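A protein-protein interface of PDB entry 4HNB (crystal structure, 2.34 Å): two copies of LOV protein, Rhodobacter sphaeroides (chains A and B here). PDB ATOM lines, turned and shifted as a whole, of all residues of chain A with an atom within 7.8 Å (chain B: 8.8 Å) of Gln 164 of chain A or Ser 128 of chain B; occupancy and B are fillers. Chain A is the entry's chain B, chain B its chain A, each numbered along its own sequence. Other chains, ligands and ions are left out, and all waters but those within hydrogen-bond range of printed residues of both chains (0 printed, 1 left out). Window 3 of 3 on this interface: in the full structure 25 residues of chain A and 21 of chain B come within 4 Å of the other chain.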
ATOM      1  N   GLN A  83     -10.686  10.608   6.873  1.00  0.00           N
ATOM      2  CA  GLN A  83     -11.701  11.102   5.964  1.00  0.00           C
ATOM      3  C   GLN A  83     -12.334   9.911   5.221  1.00  0.00           C
ATOM      4  O   GLN A  83     -11.623   9.028   4.732  1.00  0.00           O
ATOM      5  CB  GLN A  83     -11.147  12.142   4.986  1.00  0.00           C
ATOM      6  CG  GLN A  83     -10.366  13.289   5.630  1.00  0.00           C
ATOM      7  CD  GLN A  83      -8.947  12.875   5.940  1.00  0.00           C
ATOM      8  OE1 GLN A  83      -8.283  12.281   5.103  1.00  0.00           O
ATOM      9  NE2 GLN A  83      -8.495  13.136   7.162  1.00  0.00           N
ATOM     10  N   GLU A 130     -14.039  18.883  -6.256  1.00  0.00           N
ATOM     11  CA  GLU A 130     -12.690  18.915  -5.684  1.00  0.00           C
ATOM     12  C   GLU A 130     -12.344  20.246  -5.021  1.00  0.00           C
ATOM     13  O   GLU A 130     -11.806  20.278  -3.916  1.00  0.00           O
ATOM     14  CB  GLU A 130     -11.646  18.634  -6.761  1.00  0.00           C
ATOM     15  CG  GLU A 130     -11.477  17.181  -7.096  1.00  0.00           C
ATOM     16  CD  GLU A 130     -10.736  17.003  -8.387  1.00  0.00           C
ATOM     17  OE1 GLU A 130     -11.390  17.099  -9.446  1.00  0.00           O
ATOM     18  OE2 GLU A 130      -9.504  16.779  -8.342  1.00  0.00           O
ATOM     19  N   ALA A 133     -14.626  20.850  -1.934  1.00  0.00           N
ATOM     20  CA  ALA A 133     -14.223  19.969  -0.853  1.00  0.00           C
ATOM     21  C   ALA A 133     -12.931  20.490  -0.240  1.00  0.00           C
ATOM     22  O   ALA A 133     -12.765  20.480   0.982  1.00  0.00           O
ATOM     23  CB  ALA A 133     -14.021  18.560  -1.374  1.00  0.00           C
ATOM     24  N   ALA A 134     -12.023  20.938  -1.102  1.00  0.00           N
ATOM     25  CA  ALA A 134     -10.717  21.422  -0.660  1.00  0.00           C
ATOM     26  C   ALA A 134     -10.890  22.732   0.081  1.00  0.00           C
ATOM     27  O   ALA A 134     -10.261  22.942   1.119  1.00  0.00           O
ATOM     28  CB  ALA A 134      -9.764  21.587  -1.848  1.00  0.00           C
ATOM     29  N   ALA A 137     -12.035  21.860   3.431  1.00  0.00           N
ATOM     30  CA  ALA A 137     -10.894  21.366   4.198  1.00  0.00           C
ATOM     31  C   ALA A 137     -10.115  22.519   4.820  1.00  0.00           C
ATOM     32  O   ALA A 137      -9.689  22.428   5.977  1.00  0.00           O
ATOM     33  CB  ALA A 137      -9.992  20.531   3.329  1.00  0.00           C
ATOM     34  N   ASP A 157       0.505  23.333   6.872  1.00  0.00           N
ATOM     35  CA  ASP A 157       0.882  22.001   6.439  1.00  0.00           C
ATOM     36  C   ASP A 157      -0.314  21.068   6.606  1.00  0.00           C
ATOM     37  O   ASP A 157      -0.565  20.201   5.769  1.00  0.00           O
ATOM     38  CB  ASP A 157       2.091  21.510   7.233  1.00  0.00           C
ATOM     39  CG  ASP A 157       2.528  20.116   6.834  1.00  0.00           C
ATOM     40  OD1 ASP A 157       2.294  19.174   7.627  1.00  0.00           O
ATOM     41  OD2 ASP A 157       3.104  19.963   5.734  1.00  0.00           O
ATOM     42  N   SER A 158      -1.069  21.278   7.676  1.00  0.00           N
ATOM     43  CA  SER A 158      -2.267  20.497   7.922  1.00  0.00           C
ATOM     44  C   SER A 158      -3.291  20.720   6.800  1.00  0.00           C
ATOM     45  O   SER A 158      -3.799  19.758   6.216  1.00  0.00           O
ATOM     46  CB  SER A 158      -2.851  20.855   9.290  1.00  0.00           C
ATOM     47  OG  SER A 158      -3.228  19.694   9.994  1.00  0.00           O
ATOM     48  N   ARG A 159      -3.564  21.991   6.500  1.00  0.00           N
ATOM     49  CA  ARG A 159      -4.490  22.381   5.435  1.00  0.00           C
ATOM     50  C   ARG A 159      -4.144  21.757   4.088  1.00  0.00           C
ATOM     51  O   ARG A 159      -4.995  21.173   3.414  1.00  0.00           O
ATOM     52  CB  ARG A 159      -4.484  23.894   5.273  1.00  0.00           C
ATOM     53  CG  ARG A 159      -5.298  24.376   4.087  1.00  0.00           C
ATOM     54  CD  ARG A 159      -4.946  25.818   3.742  1.00  0.00           C
ATOM     55  NE  ARG A 159      -4.877  26.619   4.953  1.00  0.00           N
ATOM     56  CZ  ARG A 159      -3.875  27.427   5.272  1.00  0.00           C
ATOM     57  NH1 ARG A 159      -2.837  27.579   4.457  1.00  0.00           N
ATOM     58  NH2 ARG A 159      -3.933  28.096   6.413  1.00  0.00           N
ATOM     59  N   ARG A 160      -2.884  21.896   3.701  1.00  0.00           N
ATOM     60  CA  ARG A 160      -2.395  21.302   2.461  1.00  0.00           C
ATOM     61  C   ARG A 160      -2.649  19.792   2.386  1.00  0.00           C
ATOM     62  O   ARG A 160      -3.040  19.288   1.346  1.00  0.00           O
ATOM     63  CB  ARG A 160      -0.907  21.613   2.256  1.00  0.00           C
ATOM     64  CG  ARG A 160      -0.602  23.096   2.185  1.00  0.00           C
ATOM     65  CD  ARG A 160       0.873  23.389   2.486  1.00  0.00           C
ATOM     66  NE  ARG A 160       1.769  22.613   1.636  1.00  0.00           N
ATOM     67  CZ  ARG A 160       1.949  22.852   0.338  1.00  0.00           C
ATOM     68  NH1 ARG A 160       2.792  22.094  -0.359  1.00  0.00           N
ATOM     69  NH2 ARG A 160       1.285  23.850  -0.259  1.00  0.00           N
ATOM     70  N   HIS A 161      -2.438  19.062   3.470  1.00  0.00           N
ATOM     71  CA  HIS A 161      -2.649  17.629   3.383  1.00  0.00           C
ATOM     72  C   HIS A 161      -4.138  17.289   3.439  1.00  0.00           C
ATOM     73  O   HIS A 161      -4.595  16.372   2.755  1.00  0.00           O
ATOM     74  CB  HIS A 161      -1.814  16.869   4.415  1.00  0.00           C
ATOM     75  CG  HIS A 161      -0.342  16.862   4.094  1.00  0.00           C
ATOM     76  ND1 HIS A 161       0.478  17.926   4.365  1.00  0.00           N
ATOM     77  CD2 HIS A 161       0.430  15.919   3.496  1.00  0.00           C
ATOM     78  CE1 HIS A 161       1.713  17.643   3.963  1.00  0.00           C
ATOM     79  NE2 HIS A 161       1.704  16.437   3.434  1.00  0.00           N
ATOM     80  N   LEU A 162      -4.898  18.064   4.208  1.00  0.00           N
ATOM     81  CA  LEU A 162      -6.327  17.802   4.343  1.00  0.00           C
ATOM     82  C   LEU A 162      -7.087  18.154   3.053  1.00  0.00           C
ATOM     83  O   LEU A 162      -8.038  17.470   2.687  1.00  0.00           O
ATOM     84  CB  LEU A 162      -6.908  18.539   5.552  1.00  0.00           C
ATOM     85  CG  LEU A 162      -8.133  17.846   6.142  1.00  0.00           C
ATOM     86  CD1 LEU A 162      -7.750  16.482   6.733  1.00  0.00           C
ATOM     87  CD2 LEU A 162      -8.822  18.730   7.190  1.00  0.00           C
ATOM     88  N   ALA A 163      -6.642  19.208   2.366  1.00  0.00           N
ATOM     89  CA  ALA A 163      -7.250  19.636   1.104  1.00  0.00           C
ATOM     90  C   ALA A 163      -7.001  18.605   0.011  1.00  0.00           C
ATOM     91  O   ALA A 163      -7.897  18.268  -0.770  1.00  0.00           O
ATOM     92  CB  ALA A 163      -6.699  20.988   0.681  1.00  0.00           C
ATOM     93  N   GLN A 164      -5.766  18.123  -0.038  1.00  0.00           N
ATOM     94  CA  GLN A 164      -5.367  17.067  -0.953  1.00  0.00           C
ATOM     95  C   GLN A 164      -6.179  15.793  -0.708  1.00  0.00           C
ATOM     96  O   GLN A 164      -6.742  15.215  -1.634  1.00  0.00           O
ATOM     97  CB  GLN A 164      -3.867  16.817  -0.775  1.00  0.00           C
ATOM     98  CG  GLN A 164      -3.311  15.539  -1.361  1.00  0.00           C
ATOM     99  CD  GLN A 164      -1.792  15.443  -1.178  1.00  0.00           C
ATOM    100  OE1 GLN A 164      -1.289  15.245  -0.064  1.00  0.00           O
ATOM    101  NE2 GLN A 164      -1.054  15.608  -2.273  1.00  0.00           N
ATOM    102  N   ALA A 165      -6.246  15.371   0.549  1.00  0.00           N
ATOM    103  CA  ALA A 165      -7.018  14.201   0.932  1.00  0.00           C
ATOM    104  C   ALA A 165      -8.482  14.333   0.525  1.00  0.00           C
ATOM    105  O   ALA A 165      -9.125  13.333   0.163  1.00  0.00           O
ATOM    106  CB  ALA A 165      -6.915  13.974   2.414  1.00  0.00           C
ATOM    107  N   ALA A 166      -9.012  15.557   0.586  1.00  0.00           N
ATOM    108  CA  ALA A 166     -10.426  15.774   0.259  1.00  0.00           C
ATOM    109  C   ALA A 166     -10.636  15.656  -1.247  1.00  0.00           C
ATOM    110  O   ALA A 166     -11.565  14.981  -1.707  1.00  0.00           O
ATOM    111  CB  ALA A 166     -10.896  17.114   0.764  1.00  0.00           C
ATOM    112  N   ALA A 167      -9.762  16.305  -2.015  1.00  0.00           N
ATOM    113  CA  ALA A 167      -9.829  16.232  -3.477  1.00  0.00           C
ATOM    114  C   ALA A 167      -9.712  14.784  -3.998  1.00  0.00           C
ATOM    115  O   ALA A 167     -10.443  14.377  -4.907  1.00  0.00           O
ATOM    116  CB  ALA A 167      -8.753  17.123  -4.103  1.00  0.00           C
ATOM    117  N   ALA A 168      -8.784  14.018  -3.428  1.00  0.00           N
ATOM    118  CA  ALA A 168      -8.650  12.603  -3.769  1.00  0.00           C
ATOM    119  C   ALA A 168      -9.971  11.870  -3.531  1.00  0.00           C
ATOM    120  O   ALA A 168     -10.476  11.177  -4.420  1.00  0.00           O
ATOM    121  CB  ALA A 168      -7.528  11.956  -2.962  1.00  0.00           C
ATOM    122  N   LEU A 169     -10.541  12.039  -2.341  1.00  0.00           N
ATOM    123  CA  LEU A 169     -11.781  11.346  -2.003  1.00  0.00           C
ATOM    124  C   LEU A 169     -12.901  11.723  -2.948  1.00  0.00           C
ATOM    125  O   LEU A 169     -13.674  10.860  -3.361  1.00  0.00           O
ATOM    126  CB  LEU A 169     -12.199  11.602  -0.554  1.00  0.00           C
ATOM    127  CG  LEU A 169     -12.085  10.417   0.403  1.00  0.00           C
ATOM    128  CD1 LEU A 169     -11.420   9.226  -0.252  1.00  0.00           C
ATOM    129  CD2 LEU A 169     -11.335  10.813   1.670  1.00  0.00           C
ATOM    130  N   VAL A 170     -12.984  13.002  -3.306  1.00  0.00           N
ATOM    131  CA  VAL A 170     -14.000  13.410  -4.260  1.00  0.00           C
ATOM    132  C   VAL A 170     -13.793  12.655  -5.562  1.00  0.00           C
ATOM    133  O   VAL A 170     -14.712  12.004  -6.056  1.00  0.00           O
ATOM    134  CB  VAL A 170     -14.001  14.925  -4.512  1.00  0.00           C
ATOM    135  CG1 VAL A 170     -14.825  15.248  -5.746  1.00  0.00           C
ATOM    136  CG2 VAL A 170     -14.577  15.646  -3.311  1.00  0.00           C
ATOM    137  N   ARG A 171     -12.565  12.701  -6.077  1.00  0.00           N
ATOM    138  CA  ARG A 171     -12.211  12.018  -7.323  1.00  0.00           C
ATOM    139  C   ARG A 171     -12.589  10.532  -7.353  1.00  0.00           C
ATOM    140  O   ARG A 171     -13.069  10.041  -8.372  1.00  0.00           O
ATOM    141  CB  ARG A 171     -10.723  12.197  -7.645  1.00  0.00           C
ATOM    142  CG  ARG A 171     -10.340  13.626  -8.001  1.00  0.00           C
ATOM    143  CD  ARG A 171      -8.984  13.682  -8.691  1.00  0.00           C
ATOM    144  NE  ARG A 171      -7.886  13.238  -7.833  1.00  0.00           N
ATOM    145  CZ  ARG A 171      -7.228  14.037  -6.992  1.00  0.00           C
ATOM    146  NH1 ARG A 171      -7.568  15.321  -6.870  1.00  0.00           N
ATOM    147  NH2 ARG A 171      -6.233  13.552  -6.263  1.00  0.00           N
ATOM    148  N   PHE B 120      -0.593  33.238  -1.693  1.00  0.00           N
ATOM    149  CA  PHE B 120      -0.484  31.789  -1.730  1.00  0.00           C
ATOM    150  C   PHE B 120       0.685  31.416  -2.619  1.00  0.00           C
ATOM    151  O   PHE B 120       0.683  31.735  -3.808  1.00  0.00           O
ATOM    152  CB  PHE B 120      -1.774  31.144  -2.283  1.00  0.00           C
ATOM    153  CG  PHE B 120      -1.625  29.669  -2.608  1.00  0.00           C
ATOM    154  CD1 PHE B 120      -1.392  29.240  -3.910  1.00  0.00           C
ATOM    155  CD2 PHE B 120      -1.689  28.717  -1.596  1.00  0.00           C
ATOM    156  CE1 PHE B 120      -1.237  27.888  -4.198  1.00  0.00           C
ATOM    157  CE2 PHE B 120      -1.536  27.359  -1.875  1.00  0.00           C
ATOM    158  CZ  PHE B 120      -1.313  26.945  -3.177  1.00  0.00           C
ATOM    159  N   GLU B 121       1.685  30.736  -2.068  1.00  0.00           N
ATOM    160  CA  GLU B 121       2.815  30.356  -2.907  1.00  0.00           C
ATOM    161  C   GLU B 121       2.466  29.176  -3.814  1.00  0.00           C
ATOM    162  O   GLU B 121       2.055  28.103  -3.346  1.00  0.00           O
ATOM    163  CB  GLU B 121       4.086  30.091  -2.089  1.00  0.00           C
ATOM    164  CG  GLU B 121       5.334  29.818  -2.952  1.00  0.00           C
ATOM    165  CD  GLU B 121       6.624  29.799  -2.139  1.00  0.00           C
ATOM    166  OE1 GLU B 121       7.557  29.039  -2.488  1.00  0.00           O
ATOM    167  OE2 GLU B 121       6.700  30.548  -1.145  1.00  0.00           O
ATOM    168  N   LEU B 122       2.610  29.411  -5.118  1.00  0.00           N
ATOM    169  CA  LEU B 122       2.435  28.391  -6.137  1.00  0.00           C
ATOM    170  C   LEU B 122       3.748  27.627  -6.336  1.00  0.00           C
ATOM    171  O   LEU B 122       4.829  28.164  -6.087  1.00  0.00           O
ATOM    172  CB  LEU B 122       2.008  29.038  -7.465  1.00  0.00           C
ATOM    173  CG  LEU B 122       0.601  29.635  -7.628  1.00  0.00           C
ATOM    174  CD1 LEU B 122       0.601  30.838  -8.573  1.00  0.00           C
ATOM    175  CD2 LEU B 122      -0.378  28.582  -8.132  1.00  0.00           C
ATOM    176  N   GLY B 123       3.648  26.376  -6.783  1.00  0.00           N
ATOM    177  CA  GLY B 123       4.808  25.604  -7.190  1.00  0.00           C
ATOM    178  C   GLY B 123       5.494  24.841  -6.074  1.00  0.00           C
ATOM    179  O   GLY B 123       6.585  24.296  -6.258  1.00  0.00           O
ATOM    180  N   ARG B 124       4.867  24.814  -4.905  1.00  0.00           N
ATOM    181  CA  ARG B 124       5.370  24.014  -3.795  1.00  0.00           C
ATOM    182  C   ARG B 124       4.281  23.049  -3.345  1.00  0.00           C
ATOM    183  O   ARG B 124       4.156  22.756  -2.159  1.00  0.00           O
ATOM    184  CB  ARG B 124       5.835  24.904  -2.625  1.00  0.00           C
ATOM    185  CG  ARG B 124       4.767  25.867  -2.087  1.00  0.00           C
ATOM    186  CD  ARG B 124       5.209  26.585  -0.803  1.00  0.00           C
ATOM    187  NE  ARG B 124       5.571  25.661   0.279  1.00  0.00           N
ATOM    188  CZ  ARG B 124       4.820  25.438   1.361  1.00  0.00           C
ATOM    189  NH1 ARG B 124       3.663  26.076   1.506  1.00  0.00           N
ATOM    190  NH2 ARG B 124       5.223  24.584   2.305  1.00  0.00           N
ATOM    191  N   SER B 125       3.485  22.564  -4.295  1.00  0.00           N
ATOM    192  CA  SER B 125       2.357  21.685  -3.969  1.00  0.00           C
ATOM    193  C   SER B 125       2.209  20.500  -4.925  1.00  0.00           C
ATOM    194  O   SER B 125       1.162  19.849  -4.944  1.00  0.00           O
ATOM    195  CB  SER B 125       1.043  22.471  -3.925  1.00  0.00           C
ATOM    196  OG  SER B 125       1.051  23.432  -2.889  1.00  0.00           O
ATOM    197  N   GLY B 126       3.248  20.236  -5.718  1.00  0.00           N
ATOM    198  CA  GLY B 126       3.312  19.051  -6.560  1.00  0.00           C
ATOM    199  C   GLY B 126       2.147  18.873  -7.511  1.00  0.00           C
ATOM    200  O   GLY B 126       1.873  19.746  -8.331  1.00  0.00           O
ATOM    201  N   ASN B 127       1.452  17.743  -7.389  1.00  0.00           N
ATOM    202  CA  ASN B 127       0.297  17.442  -8.236  1.00  0.00           C
ATOM    203  C   ASN B 127      -1.036  18.034  -7.762  1.00  0.00           C
ATOM    204  O   ASN B 127      -2.046  17.941  -8.467  1.00  0.00           O
ATOM    205  CB  ASN B 127       0.137  15.930  -8.394  1.00  0.00           C
ATOM    206  CG  ASN B 127       1.180  15.323  -9.308  1.00  0.00           C
ATOM    207  OD1 ASN B 127       1.113  15.473 -10.531  1.00  0.00           O
ATOM    208  ND2 ASN B 127       2.142  14.617  -8.723  1.00  0.00           N
ATOM    209  N   SER B 128      -1.056  18.630  -6.576  1.00  0.00           N
ATOM    210  CA  SER B 128      -2.314  19.165  -6.056  1.00  0.00           C
ATOM    211  C   SER B 128      -2.282  20.665  -5.784  1.00  0.00           C
ATOM    212  O   SER B 128      -2.652  21.112  -4.699  1.00  0.00           O
ATOM    213  CB  SER B 128      -2.774  18.395  -4.811  1.00  0.00           C
ATOM    214  OG  SER B 128      -1.704  18.138  -3.922  1.00  0.00           O
ATOM    215  N   GLU B 129      -1.856  21.440  -6.777  1.00  0.00           N
ATOM    216  CA  GLU B 129      -1.863  22.895  -6.654  1.00  0.00           C
ATOM    217  C   GLU B 129      -3.290  23.401  -6.510  1.00  0.00           C
ATOM    218  O   GLU B 129      -3.570  24.240  -5.661  1.00  0.00           O
ATOM    219  CB  GLU B 129      -1.174  23.558  -7.856  1.00  0.00           C
ATOM    220  CG  GLU B 129       0.321  23.263  -7.976  1.00  0.00           C
ATOM    221  CD  GLU B 129       1.188  24.079  -7.024  1.00  0.00           C
ATOM    222  OE1 GLU B 129       0.737  25.135  -6.514  1.00  0.00           O
ATOM    223  OE2 GLU B 129       2.336  23.650  -6.780  1.00  0.00           O
ATOM    224  N   GLU B 130      -4.184  22.892  -7.347  1.00  0.00           N
ATOM    225  CA  GLU B 130      -5.601  23.241  -7.272  1.00  0.00           C
ATOM    226  C   GLU B 130      -6.191  23.026  -5.882  1.00  0.00           C
ATOM    227  O   GLU B 130      -6.845  23.915  -5.338  1.00  0.00           O
ATOM    228  CB  GLU B 130      -6.410  22.443  -8.298  1.00  0.00           C
ATOM    229  CG  GLU B 130      -6.328  22.997  -9.700  1.00  0.00           C
ATOM    230  CD  GLU B 130      -7.067  22.149 -10.706  1.00  0.00           C
ATOM    231  OE1 GLU B 130      -6.494  21.139 -11.167  1.00  0.00           O
ATOM    232  OE2 GLU B 130      -8.221  22.498 -11.041  1.00  0.00           O
ATOM    233  N   ALA B 131      -5.966  21.840  -5.323  1.00  0.00           N
ATOM    234  CA  ALA B 131      -6.462  21.499  -3.994  1.00  0.00           C
ATOM    235  C   ALA B 131      -5.914  22.464  -2.951  1.00  0.00           C
ATOM    236  O   ALA B 131      -6.656  22.999  -2.122  1.00  0.00           O
ATOM    237  CB  ALA B 131      -6.074  20.072  -3.636  1.00  0.00           C
ATOM    238  N   ALA B 132      -4.609  22.687  -3.008  1.00  0.00           N
ATOM    239  CA  ALA B 132      -3.947  23.549  -2.042  1.00  0.00           C
ATOM    240  C   ALA B 132      -4.422  24.992  -2.174  1.00  0.00           C
ATOM    241  O   ALA B 132      -4.585  25.686  -1.183  1.00  0.00           O
ATOM    242  CB  ALA B 132      -2.428  23.454  -2.192  1.00  0.00           C
ATOM    243  N   ALA B 133      -4.650  25.447  -3.397  1.00  0.00           N
ATOM    244  CA  ALA B 133      -5.124  26.809  -3.581  1.00  0.00           C
ATOM    245  C   ALA B 133      -6.534  26.946  -3.027  1.00  0.00           C
ATOM    246  O   ALA B 133      -6.857  27.907  -2.310  1.00  0.00           O
ATOM    247  CB  ALA B 133      -5.087  27.180  -5.053  1.00  0.00           C
ATOM    248  N   ALA B 134      -7.373  25.978  -3.384  1.00  0.00           N
ATOM    249  CA  ALA B 134      -8.753  25.918  -2.925  1.00  0.00           C
ATOM    250  C   ALA B 134      -8.809  25.846  -1.404  1.00  0.00           C
ATOM    251  O   ALA B 134      -9.631  26.507  -0.784  1.00  0.00           O
ATOM    252  CB  ALA B 134      -9.453  24.735  -3.545  1.00  0.00           C
ATOM    253  N   GLY B 135      -7.919  25.059  -0.805  1.00  0.00           N
ATOM    254  CA  GLY B 135      -7.761  25.054   0.641  1.00  0.00           C
ATOM    255  C   GLY B 135      -7.459  26.432   1.198  1.00  0.00           C
ATOM    256  O   GLY B 135      -8.138  26.895   2.120  1.00  0.00           O
ATOM    257  N   VAL B 170      -5.073  28.682 -10.946  1.00  0.00           N
ATOM    258  CA  VAL B 170      -3.975  27.732 -10.875  1.00  0.00           C
ATOM    259  C   VAL B 170      -3.828  27.004 -12.199  1.00  0.00           C
ATOM    260  O   VAL B 170      -2.721  26.871 -12.723  1.00  0.00           O
ATOM    261  CB  VAL B 170      -4.207  26.717  -9.758  1.00  0.00           C
ATOM    262  CG1 VAL B 170      -3.339  25.489  -9.963  1.00  0.00           C
ATOM    263  CG2 VAL B 170      -3.920  27.363  -8.417  1.00  0.00           C
ATOM    264  N   TRP B 173      -2.271  29.167 -14.744  1.00  0.00           N
ATOM    265  CA  TRP B 173      -0.847  29.274 -14.424  1.00  0.00           C
ATOM    266  C   TRP B 173      -0.045  28.026 -14.809  1.00  0.00           C
ATOM    267  O   TRP B 173       1.174  28.103 -14.998  1.00  0.00           O
ATOM    268  CB  TRP B 173      -0.664  29.602 -12.938  1.00  0.00           C
ATOM    269  CG  TRP B 173       0.757  29.549 -12.439  1.00  0.00           C
ATOM    270  CD1 TRP B 173       1.666  30.558 -12.448  1.00  0.00           C
ATOM    271  CD2 TRP B 173       1.414  28.429 -11.838  1.00  0.00           C
ATOM    272  NE1 TRP B 173       2.851  30.139 -11.894  1.00  0.00           N
ATOM    273  CE2 TRP B 173       2.721  28.823 -11.510  1.00  0.00           C
ATOM    274  CE3 TRP B 173       1.019  27.117 -11.541  1.00  0.00           C
ATOM    275  CZ2 TRP B 173       3.647  27.969 -10.908  1.00  0.00           C
ATOM    276  CZ3 TRP B 173       1.933  26.264 -10.942  1.00  0.00           C
ATOM    277  CH2 TRP B 173       3.234  26.694 -10.631  1.00  0.00           C
ATOM    278  N   GLU B 174      -0.724  26.885 -14.922  1.00  0.00           N
ATOM    279  CA  GLU B 174      -0.083  25.649 -15.383  1.00  0.00           C
ATOM    280  C   GLU B 174      -0.205  25.482 -16.903  1.00  0.00           C
ATOM    281  O   GLU B 174       0.513  24.686 -17.510  1.00  0.00           O
ATOM    282  CB  GLU B 174      -0.648  24.422 -14.651  1.00  0.00           C
ATOM    283  CG  GLU B 174      -0.373  24.423 -13.147  1.00  0.00           C
ATOM    284  CD  GLU B 174      -1.007  23.250 -12.400  1.00  0.00           C
ATOM    285  OE1 GLU B 174      -1.919  22.587 -12.945  1.00  0.00           O
ATOM    286  OE2 GLU B 174      -0.583  22.995 -11.253  1.00  0.00           O
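NH1 of Arg 160 of chain A lies close to O of Arg 124 of chain B, 2.4 Å away.
OG of Ser 128 of chain B is in hydrogen-bond range of NE2 of Gln 164 of chain A (3.1 Å).
The guanidinium group of Arg 160 of chain A is in hydrogen-bond range of the side-chain hydroxyl of Ser 125 of chain B.
The backbone NH of Arg 124 of chain B sits at hydrogen-bond distance from the side-chain carboxylate of Glu 129 of chain B, 3.4 Å away.
O of Ser 125 of chain B sits at hydrogen-bond distance from OG of Ser 128 of chain B (3.5 Å).
The backbone NH (N) of Ser 125 of chain B sits at hydrogen-bond distance from the side-chain carboxylate (OE2) of Glu 129 of chain B (2.9 Å).
Ala 134 of chain A touches Ala 131 of chain B (CB to O, 3.4 Å).
Ala 134 of chain B touches Ala 134 of chain A.
Ala 134 of chain A touches Gly 135 of chain B (O to CA, 3.3 Å).
Gly 135 of chain B touches Arg 159 of chain A.
Ala 163 of chain A touches Ala 131 of chain B (CB to O, 3.5 Å).
Of the printed residues of chain B, Ala 134 of chain A touches Ala 131 (3.4 Å), Ala 134 (3.6 Å) and Gly 135 (3.3 Å).
Of chain B, only Ala 131 comes within 4 Å of Ala 163 of chain A.
Gln 164 of chain A touches one residue of chain B.
No residue of chain B comes within 4 Å of Ala 165 of chain A.
Ala 167 of chain A touches none of the printed residues of chain B.
Of the printed residues of chain A, Arg 124 of chain B touches Arg 160.
Of chain A, only Gln 164 (3.1 Å) comes within 4 Å of Ser 128 of chain B.
Of the printed residues of chain A, Ala 131 of chain B touches Ala 134 (3.4 Å) and Ala 163 (3.5 Å).
Printed residues of chain A within 4 Å of Ala 134 of chain B: Ala 134.
The nearest residue of chain B that does not touch Gln 164 of chain A is Ala 131 of chain B (4.1 Å).
The nearest residue of chain A that does not touch Ser 128 of chain B is Arg 160 of chain A (5.6 Å).
The nearest printed residue of chain A that does not touch Gly 135 of chain B is Ala 163 of chain A (4.2 Å).
Of the 20 printed residues of chain A, 5 touch a printed residue of chain B.
Printed residues of chain A that touch a printed residue of chain B: Ala 134, Arg 159, Arg 160, Ala 163 and Gln 164.
Among the printed residues, 8 pairs touch across the chains.
Among the printed residues, no Asp or Glu carboxylate lies within 4 Å of a Lys or Arg side-chain nitrogen of the other chain.
Ala 134 of chain B touches its own counterpart, Ala 134 of chain A.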
